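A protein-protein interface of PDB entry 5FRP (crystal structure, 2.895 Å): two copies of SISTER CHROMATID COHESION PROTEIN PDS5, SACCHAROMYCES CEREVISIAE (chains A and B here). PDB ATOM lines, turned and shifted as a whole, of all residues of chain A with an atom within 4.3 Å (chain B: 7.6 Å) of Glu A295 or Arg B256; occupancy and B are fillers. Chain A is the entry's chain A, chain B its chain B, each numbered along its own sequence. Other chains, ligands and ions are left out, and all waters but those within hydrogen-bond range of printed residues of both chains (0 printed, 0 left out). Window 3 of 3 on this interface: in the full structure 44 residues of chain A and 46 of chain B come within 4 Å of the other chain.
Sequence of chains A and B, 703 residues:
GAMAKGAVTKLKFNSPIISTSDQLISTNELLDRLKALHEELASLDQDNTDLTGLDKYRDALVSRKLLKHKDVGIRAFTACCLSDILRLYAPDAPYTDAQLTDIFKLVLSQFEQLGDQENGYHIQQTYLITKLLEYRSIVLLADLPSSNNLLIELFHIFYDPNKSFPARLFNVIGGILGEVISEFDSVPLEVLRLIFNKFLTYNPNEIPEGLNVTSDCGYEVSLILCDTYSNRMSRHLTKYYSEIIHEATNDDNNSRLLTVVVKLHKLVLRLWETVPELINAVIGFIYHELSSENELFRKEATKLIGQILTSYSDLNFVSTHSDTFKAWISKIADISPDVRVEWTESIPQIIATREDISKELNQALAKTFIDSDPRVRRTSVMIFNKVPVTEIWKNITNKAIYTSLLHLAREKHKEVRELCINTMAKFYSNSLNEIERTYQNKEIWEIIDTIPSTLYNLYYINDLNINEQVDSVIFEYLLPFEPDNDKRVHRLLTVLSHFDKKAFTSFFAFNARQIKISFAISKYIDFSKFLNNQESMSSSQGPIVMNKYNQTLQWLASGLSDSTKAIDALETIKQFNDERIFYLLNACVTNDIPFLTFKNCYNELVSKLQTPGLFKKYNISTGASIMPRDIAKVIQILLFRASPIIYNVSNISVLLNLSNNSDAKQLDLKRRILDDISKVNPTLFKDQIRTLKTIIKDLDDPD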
ATOM      1  N   GLU A 293       8.222  10.038 -32.359  1.00  0.00           N
ATOM      2  CA  GLU A 293       8.042  11.185 -31.476  1.00  0.00           C
ATOM      3  C   GLU A 293       9.377  11.801 -31.068  1.00  0.00           C
ATOM      4  O   GLU A 293       9.496  13.022 -30.965  1.00  0.00           O
ATOM      5  CB  GLU A 293       7.250  10.789 -30.229  1.00  0.00           C
ATOM      6  CG  GLU A 293       5.758  10.615 -30.478  1.00  0.00           C
ATOM      7  CD  GLU A 293       5.047  11.915 -30.814  1.00  0.00           C
ATOM      8  OE1 GLU A 293       4.955  12.786 -29.923  1.00  0.00           O
ATOM      9  OE2 GLU A 293       4.570  12.071 -31.958  1.00  0.00           O
ATOM     10  N   ASN A 294      10.374  10.955 -30.832  1.00  0.00           N
ATOM     11  CA  ASN A 294      11.681  11.417 -30.381  1.00  0.00           C
ATOM     12  C   ASN A 294      12.481  11.906 -31.584  1.00  0.00           C
ATOM     13  O   ASN A 294      12.729  11.148 -32.522  1.00  0.00           O
ATOM     14  CB  ASN A 294      12.412  10.286 -29.661  1.00  0.00           C
ATOM     15  CG  ASN A 294      13.548  10.773 -28.788  1.00  0.00           C
ATOM     16  OD1 ASN A 294      14.240  11.736 -29.123  1.00  0.00           O
ATOM     17  ND2 ASN A 294      13.748  10.108 -27.656  1.00  0.00           N
ATOM     18  N   GLU A 295      12.896  13.169 -31.542  1.00  0.00           N
ATOM     19  CA  GLU A 295      13.592  13.785 -32.668  1.00  0.00           C
ATOM     20  C   GLU A 295      14.881  13.045 -33.014  1.00  0.00           C
ATOM     21  O   GLU A 295      15.204  12.875 -34.188  1.00  0.00           O
ATOM     22  CB  GLU A 295      13.896  15.261 -32.382  1.00  0.00           C
ATOM     23  CG  GLU A 295      14.635  15.523 -31.077  1.00  0.00           C
ATOM     24  CD  GLU A 295      15.049  16.974 -30.913  1.00  0.00           C
ATOM     25  OE1 GLU A 295      14.428  17.856 -31.543  1.00  0.00           O
ATOM     26  OE2 GLU A 295      16.002  17.232 -30.147  1.00  0.00           O
ATOM     27  N   LEU A 296      15.611  12.605 -31.994  1.00  0.00           N
ATOM     28  CA  LEU A 296      16.914  11.978 -32.197  1.00  0.00           C
ATOM     29  C   LEU A 296      16.826  10.769 -33.129  1.00  0.00           C
ATOM     30  O   LEU A 296      17.665  10.602 -34.020  1.00  0.00           O
ATOM     31  CB  LEU A 296      17.519  11.554 -30.857  1.00  0.00           C
ATOM     32  CG  LEU A 296      17.766  12.683 -29.851  1.00  0.00           C
ATOM     33  CD1 LEU A 296      18.063  12.101 -28.483  1.00  0.00           C
ATOM     34  CD2 LEU A 296      18.904  13.581 -30.311  1.00  0.00           C
ATOM     35  N   PHE A 297      15.810   9.936 -32.936  1.00  0.00           N
ATOM     36  CA  PHE A 297      15.653   8.754 -33.772  1.00  0.00           C
ATOM     37  C   PHE A 297      15.285   9.142 -35.203  1.00  0.00           C
ATOM     38  O   PHE A 297      15.706   8.481 -36.156  1.00  0.00           O
ATOM     39  CB  PHE A 297      14.599   7.817 -33.184  1.00  0.00           C
ATOM     40  CG  PHE A 297      14.982   7.258 -31.843  1.00  0.00           C
ATOM     41  CD1 PHE A 297      16.161   6.554 -31.685  1.00  0.00           C
ATOM     42  CD2 PHE A 297      14.159   7.429 -30.747  1.00  0.00           C
ATOM     43  CE1 PHE A 297      16.517   6.038 -30.455  1.00  0.00           C
ATOM     44  CE2 PHE A 297      14.506   6.916 -29.515  1.00  0.00           C
ATOM     45  CZ  PHE A 297      15.688   6.219 -29.368  1.00  0.00           C
ATOM     46  N   ARG A 298      14.509  10.211 -35.358  1.00  0.00           N
ATOM     47  CA  ARG A 298      14.251  10.760 -36.686  1.00  0.00           C
ATOM     48  C   ARG A 298      15.563  11.213 -37.311  1.00  0.00           C
ATOM     49  O   ARG A 298      15.834  10.924 -38.477  1.00  0.00           O
ATOM     50  CB  ARG A 298      13.262  11.928 -36.619  1.00  0.00           C
ATOM     51  CG  ARG A 298      11.906  11.532 -36.052  1.00  0.00           C
ATOM     52  CD  ARG A 298      10.883  12.664 -36.130  1.00  0.00           C
ATOM     53  NE  ARG A 298      11.487  13.982 -35.953  1.00  0.00           N
ATOM     54  CZ  ARG A 298      10.966  14.968 -35.225  1.00  0.00           C
ATOM     55  NH1 ARG A 298       9.822  14.801 -34.573  1.00  0.00           N
ATOM     56  NH2 ARG A 298      11.602  16.126 -35.143  1.00  0.00           N
ATOM     57  N   LYS A 299      16.371  11.918 -36.523  1.00  0.00           N
ATOM     58  CA  LYS A 299      17.666  12.402 -36.978  1.00  0.00           C
ATOM     59  C   LYS A 299      18.483  11.232 -37.504  1.00  0.00           C
ATOM     60  O   LYS A 299      18.972  11.263 -38.639  1.00  0.00           O
ATOM     61  CB  LYS A 299      18.407  13.102 -35.836  1.00  0.00           C
ATOM     62  CG  LYS A 299      19.686  13.803 -36.261  1.00  0.00           C
ATOM     63  CD  LYS A 299      20.379  14.439 -35.067  1.00  0.00           C
ATOM     64  CE  LYS A 299      21.707  15.064 -35.467  1.00  0.00           C
ATOM     65  NZ  LYS A 299      22.463  15.542 -34.272  1.00  0.00           N
ATOM     66  N   SER A 336      12.046  19.612 -35.901  1.00  0.00           N
ATOM     67  CA  SER A 336      13.375  19.743 -35.311  1.00  0.00           C
ATOM     68  C   SER A 336      14.400  20.221 -36.341  1.00  0.00           C
ATOM     69  O   SER A 336      14.656  19.530 -37.328  1.00  0.00           O
ATOM     70  CB  SER A 336      13.821  18.406 -34.722  1.00  0.00           C
ATOM     71  OG  SER A 336      15.195  18.444 -34.376  1.00  0.00           O
ATOM     72  N   VAL A 339      17.166  17.873 -37.526  1.00  0.00           N
ATOM     73  CA  VAL A 339      16.789  16.905 -38.546  1.00  0.00           C
ATOM     74  C   VAL A 339      16.985  17.532 -39.921  1.00  0.00           C
ATOM     75  O   VAL A 339      17.564  16.912 -40.816  1.00  0.00           O
ATOM     76  CB  VAL A 339      15.330  16.440 -38.368  1.00  0.00           C
ATOM     77  CG1 VAL A 339      14.973  15.373 -39.395  1.00  0.00           C
ATOM     78  CG2 VAL A 339      15.115  15.913 -36.959  1.00  0.00           C
ATOM     79  N   ILE B 244      23.687  21.619 -17.102  1.00  0.00           N
ATOM     80  CA  ILE B 244      23.389  21.039 -18.402  1.00  0.00           C
ATOM     81  C   ILE B 244      23.148  19.546 -18.222  1.00  0.00           C
ATOM     82  O   ILE B 244      22.151  19.009 -18.715  1.00  0.00           O
ATOM     83  CB  ILE B 244      24.533  21.297 -19.412  1.00  0.00           C
ATOM     84  CG1 ILE B 244      24.577  22.774 -19.826  1.00  0.00           C
ATOM     85  CG2 ILE B 244      24.395  20.393 -20.634  1.00  0.00           C
ATOM     86  CD1 ILE B 244      23.381  23.253 -20.640  1.00  0.00           C
ATOM     87  N   GLU B 247      19.845  18.961 -16.356  1.00  0.00           N
ATOM     88  CA  GLU B 247      18.699  19.187 -17.226  1.00  0.00           C
ATOM     89  C   GLU B 247      18.540  18.015 -18.184  1.00  0.00           C
ATOM     90  O   GLU B 247      17.443  17.476 -18.339  1.00  0.00           O
ATOM     91  CB  GLU B 247      18.860  20.494 -18.005  1.00  0.00           C
ATOM     92  CG  GLU B 247      17.641  20.861 -18.838  1.00  0.00           C
ATOM     93  CD  GLU B 247      17.794  22.190 -19.556  1.00  0.00           C
ATOM     94  OE1 GLU B 247      18.649  22.295 -20.461  1.00  0.00           O
ATOM     95  OE2 GLU B 247      17.053  23.133 -19.206  1.00  0.00           O
ATOM     96  N   ALA B 248      19.641  17.626 -18.818  1.00  0.00           N
ATOM     97  CA  ALA B 248      19.625  16.520 -19.766  1.00  0.00           C
ATOM     98  C   ALA B 248      19.145  15.222 -19.118  1.00  0.00           C
ATOM     99  O   ALA B 248      18.356  14.485 -19.708  1.00  0.00           O
ATOM    100  CB  ALA B 248      21.008  16.326 -20.361  1.00  0.00           C
ATOM    101  N   THR B 249      19.622  14.946 -17.909  1.00  0.00           N
ATOM    102  CA  THR B 249      19.277  13.706 -17.217  1.00  0.00           C
ATOM    103  C   THR B 249      17.762  13.567 -17.067  1.00  0.00           C
ATOM    104  O   THR B 249      17.168  12.611 -17.570  1.00  0.00           O
ATOM    105  CB  THR B 249      19.948  13.654 -15.827  1.00  0.00           C
ATOM    106  OG1 THR B 249      21.362  13.818 -15.986  1.00  0.00           O
ATOM    107  CG2 THR B 249      19.679  12.324 -15.133  1.00  0.00           C
ATOM    108  N   ASN B 250      17.148  14.522 -16.376  1.00  0.00           N
ATOM    109  CA  ASN B 250      15.714  14.489 -16.092  1.00  0.00           C
ATOM    110  C   ASN B 250      14.849  14.901 -17.285  1.00  0.00           C
ATOM    111  O   ASN B 250      13.639  15.074 -17.144  1.00  0.00           O
ATOM    112  CB  ASN B 250      15.386  15.389 -14.900  1.00  0.00           C
ATOM    113  CG  ASN B 250      16.157  15.008 -13.652  1.00  0.00           C
ATOM    114  OD1 ASN B 250      16.679  13.899 -13.546  1.00  0.00           O
ATOM    115  ND2 ASN B 250      16.229  15.927 -12.697  1.00  0.00           N
ATOM    116  N   ASP B 251      15.467  15.053 -18.453  1.00  0.00           N
ATOM    117  CA  ASP B 251      14.778  15.554 -19.643  1.00  0.00           C
ATOM    118  C   ASP B 251      13.696  14.605 -20.180  1.00  0.00           C
ATOM    119  O   ASP B 251      13.133  14.850 -21.246  1.00  0.00           O
ATOM    120  CB  ASP B 251      15.807  15.839 -20.742  1.00  0.00           C
ATOM    121  CG  ASP B 251      15.208  16.573 -21.927  1.00  0.00           C
ATOM    122  OD1 ASP B 251      15.150  17.821 -21.891  1.00  0.00           O
ATOM    123  OD2 ASP B 251      14.799  15.907 -22.903  1.00  0.00           O
ATOM    124  N   ASP B 252      13.407  13.524 -19.458  1.00  0.00           N
ATOM    125  CA  ASP B 252      12.350  12.588 -19.850  1.00  0.00           C
ATOM    126  C   ASP B 252      12.775  11.797 -21.085  1.00  0.00           C
ATOM    127  O   ASP B 252      12.684  10.569 -21.102  1.00  0.00           O
ATOM    128  CB  ASP B 252      11.040  13.334 -20.120  1.00  0.00           C
ATOM    129  CG  ASP B 252       9.832  12.421 -20.059  1.00  0.00           C
ATOM    130  OD1 ASP B 252       9.272  12.244 -18.956  1.00  0.00           O
ATOM    131  OD2 ASP B 252       9.436  11.876 -21.112  1.00  0.00           O
ATOM    132  N   ASN B 253      13.225  12.501 -22.120  1.00  0.00           N
ATOM    133  CA  ASN B 253      13.873  11.853 -23.247  1.00  0.00           C
ATOM    134  C   ASN B 253      15.088  11.137 -22.679  1.00  0.00           C
ATOM    135  O   ASN B 253      15.982  11.771 -22.117  1.00  0.00           O
ATOM    136  CB  ASN B 253      14.266  12.881 -24.308  1.00  0.00           C
ATOM    137  CG  ASN B 253      14.761  12.244 -25.589  1.00  0.00           C
ATOM    138  OD1 ASN B 253      15.160  11.079 -25.606  1.00  0.00           O
ATOM    139  ND2 ASN B 253      14.734  13.006 -26.677  1.00  0.00           N
ATOM    140  N   ASN B 254      15.130   9.819 -22.831  1.00  0.00           N
ATOM    141  CA  ASN B 254      16.130   9.014 -22.141  1.00  0.00           C
ATOM    142  C   ASN B 254      17.444   8.905 -22.910  1.00  0.00           C
ATOM    143  O   ASN B 254      18.459   8.490 -22.351  1.00  0.00           O
ATOM    144  CB  ASN B 254      15.569   7.617 -21.878  1.00  0.00           C
ATOM    145  CG  ASN B 254      14.352   7.653 -20.972  1.00  0.00           C
ATOM    146  OD1 ASN B 254      14.483   7.746 -19.752  1.00  0.00           O
ATOM    147  ND2 ASN B 254      13.164   7.575 -21.564  1.00  0.00           N
ATOM    148  N   SER B 255      17.421   9.282 -24.182  1.00  0.00           N
ATOM    149  CA  SER B 255      18.608   9.209 -25.028  1.00  0.00           C
ATOM    150  C   SER B 255      19.248  10.583 -25.194  1.00  0.00           C
ATOM    151  O   SER B 255      20.118  10.772 -26.045  1.00  0.00           O
ATOM    152  CB  SER B 255      18.255   8.633 -26.399  1.00  0.00           C
ATOM    153  OG  SER B 255      17.762   7.311 -26.269  1.00  0.00           O
ATOM    154  N   ARG B 256      18.821  11.532 -24.367  1.00  0.00           N
ATOM    155  CA  ARG B 256      19.270  12.914 -24.467  1.00  0.00           C
ATOM    156  C   ARG B 256      20.639  13.078 -23.801  1.00  0.00           C
ATOM    157  O   ARG B 256      21.567  13.667 -24.376  1.00  0.00           O
ATOM    158  CB  ARG B 256      18.242  13.822 -23.788  1.00  0.00           C
ATOM    159  CG  ARG B 256      18.365  15.317 -24.060  1.00  0.00           C
ATOM    160  CD  ARG B 256      17.457  15.792 -25.198  1.00  0.00           C
ATOM    161  NE  ARG B 256      18.131  15.940 -26.483  1.00  0.00           N
ATOM    162  CZ  ARG B 256      17.519  16.294 -27.610  1.00  0.00           C
ATOM    163  NH1 ARG B 256      16.213  16.532 -27.622  1.00  0.00           N
ATOM    164  NH2 ARG B 256      18.215  16.410 -28.732  1.00  0.00           N
ATOM    165  N   LEU B 257      20.747  12.534 -22.591  1.00  0.00           N
ATOM    166  CA  LEU B 257      21.928  12.688 -21.746  1.00  0.00           C
ATOM    167  C   LEU B 257      23.219  12.404 -22.502  1.00  0.00           C
ATOM    168  O   LEU B 257      24.139  13.219 -22.491  1.00  0.00           O
ATOM    169  CB  LEU B 257      21.825  11.779 -20.520  1.00  0.00           C
ATOM    170  CG  LEU B 257      23.010  11.800 -19.549  1.00  0.00           C
ATOM    171  CD1 LEU B 257      23.390  13.225 -19.167  1.00  0.00           C
ATOM    172  CD2 LEU B 257      22.673  10.989 -18.311  1.00  0.00           C
ATOM    173  N   LEU B 258      23.291  11.241 -23.145  1.00  0.00           N
ATOM    174  CA  LEU B 258      24.492  10.858 -23.877  1.00  0.00           C
ATOM    175  C   LEU B 258      24.841  11.916 -24.923  1.00  0.00           C
ATOM    176  O   LEU B 258      25.990  12.366 -25.006  1.00  0.00           O
ATOM    177  CB  LEU B 258      24.306   9.493 -24.538  1.00  0.00           C
ATOM    178  CG  LEU B 258      25.519   8.934 -25.287  1.00  0.00           C
ATOM    179  CD1 LEU B 258      26.749   8.895 -24.393  1.00  0.00           C
ATOM    180  CD2 LEU B 258      25.202   7.546 -25.818  1.00  0.00           C
ATOM    181  N   THR B 259      23.848  12.319 -25.707  1.00  0.00           N
ATOM    182  CA  THR B 259      24.064  13.311 -26.749  1.00  0.00           C
ATOM    183  C   THR B 259      24.567  14.609 -26.128  1.00  0.00           C
ATOM    184  O   THR B 259      25.400  15.303 -26.715  1.00  0.00           O
ATOM    185  CB  THR B 259      22.779  13.600 -27.555  1.00  0.00           C
ATOM    186  OG1 THR B 259      21.808  14.219 -26.705  1.00  0.00           O
ATOM    187  CG2 THR B 259      22.195  12.318 -28.137  1.00  0.00           C
ATOM    188  N   VAL B 260      24.059  14.936 -24.943  1.00  0.00           N
ATOM    189  CA  VAL B 260      24.470  16.161 -24.263  1.00  0.00           C
ATOM    190  C   VAL B 260      25.892  16.053 -23.697  1.00  0.00           C
ATOM    191  O   VAL B 260      26.680  16.998 -23.807  1.00  0.00           O
ATOM    192  CB  VAL B 260      23.484  16.517 -23.132  1.00  0.00           C
ATOM    193  CG1 VAL B 260      23.978  17.721 -22.339  1.00  0.00           C
ATOM    194  CG2 VAL B 260      22.109  16.791 -23.704  1.00  0.00           C
ATOM    195  N   VAL B 261      26.235  14.916 -23.098  1.00  0.00           N
ATOM    196  CA  VAL B 261      27.559  14.770 -22.506  1.00  0.00           C
ATOM    197  C   VAL B 261      28.611  14.745 -23.608  1.00  0.00           C
ATOM    198  O   VAL B 261      29.681  15.344 -23.466  1.00  0.00           O
ATOM    199  CB  VAL B 261      27.653  13.508 -21.619  1.00  0.00           C
ATOM    200  CG1 VAL B 261      27.317  12.261 -22.395  1.00  0.00           C
ATOM    201  CG2 VAL B 261      29.036  13.394 -20.980  1.00  0.00           C
ATOM    202  N   VAL B 262      28.309  14.065 -24.710  1.00  0.00           N
ATOM    203  CA  VAL B 262      29.249  14.011 -25.825  1.00  0.00           C
ATOM    204  C   VAL B 262      29.491  15.421 -26.364  1.00  0.00           C
ATOM    205  O   VAL B 262      30.528  15.685 -26.974  1.00  0.00           O
ATOM    206  CB  VAL B 262      28.745  13.077 -26.947  1.00  0.00           C
ATOM    207  CG1 VAL B 262      29.656  13.156 -28.167  1.00  0.00           C
ATOM    208  CG2 VAL B 262      28.667  11.646 -26.444  1.00  0.00           C
ATOM    209  N   PHE B 297      29.623   6.324 -20.594  1.00  0.00           N
ATOM    210  CA  PHE B 297      30.159   7.598 -20.133  1.00  0.00           C
ATOM    211  C   PHE B 297      31.660   7.477 -19.856  1.00  0.00           C
ATOM    212  O   PHE B 297      32.417   8.427 -20.085  1.00  0.00           O
ATOM    213  CB  PHE B 297      29.404   8.078 -18.892  1.00  0.00           C
ATOM    214  CG  PHE B 297      27.944   8.352 -19.151  1.00  0.00           C
ATOM    215  CD1 PHE B 297      27.559   9.245 -20.135  1.00  0.00           C
ATOM    216  CD2 PHE B 297      26.965   7.719 -18.408  1.00  0.00           C
ATOM    217  CE1 PHE B 297      26.221   9.496 -20.378  1.00  0.00           C
ATOM    218  CE2 PHE B 297      25.626   7.966 -18.644  1.00  0.00           C
ATOM    219  CZ  PHE B 297      25.254   8.857 -19.630  1.00  0.00           C
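Position printed for both chains: 297.
The side-chain amide nitrogen of Asn A294 is in hydrogen-bond range of the side-chain amide oxygen of Asn B253.
The guanidinium group (NH1) of Arg B256 is in salt-bridge range of the side-chain carboxylate (OE2) of Glu A295 (2.6 Å).
Glu A295 touches one residue of chain B.
Arg B256 touches just these residues of chain A: Glu A295 (2.6 Å) and Leu A296 (3.3 Å).
Of the printed residues of chain B, Phe A297 touches Ser B255 (3.9 Å).
Printed residues of chain B within 4 Å of Leu A296: Asn B253 (3.9 Å), Ser B255 (3.5 Å) and Arg B256 (3.3 Å).
Of the printed residues of chain A, Asn B253 touches Asn A294 and Leu A296.
Printed residues of chain B within 4 Å of Asn A294: Asn B253.
Of the printed residues of chain A, Ser B255 touches Leu A296 (3.5 Å) and Phe A297 (3.9 Å).
Asp B252 touches none of the printed residues of chain A.
Glu B247 touches none of the printed residues of chain A.
Asn B253 touches Leu A296.
O of Ser B255 touches CD1 of Leu A296, at 3.5 Å.
Leu A296 touches Arg B256.
Ser B255 touches Phe A297 (OG to CZ, 3.9 Å).
The side-chain amide oxygen of Asn A294 lies close to the backbone NH of Leu A296, at 3.3 Å.
The backbone carbonyl oxygen of Arg B256 is in hydrogen-bond range of the side-chain hydroxyl of Thr B259, 2.4 Å away.
OG of Ser A336 lies within hydrogen-bond range of OE1 of Glu A295 (3.0 Å).
The backbone NH (N) of Ser B255 sits at hydrogen-bond distance from the side-chain amide oxygen (OD1) of Asn B253, at 3.2 Å.
Hydrophobic or aromatic side chains of chain A within 4 Å of the printed part of chain B: Leu A296 and Phe A297.
Printed residues of chain B that touch a printed residue of chain A: Asn B253, Ser B255 and Arg B256.
Among the printed residues, Asp or Glu carboxylates within 4 Å of a Lys or Arg side-chain nitrogen of the other chain: Glu A295 with Arg B256.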
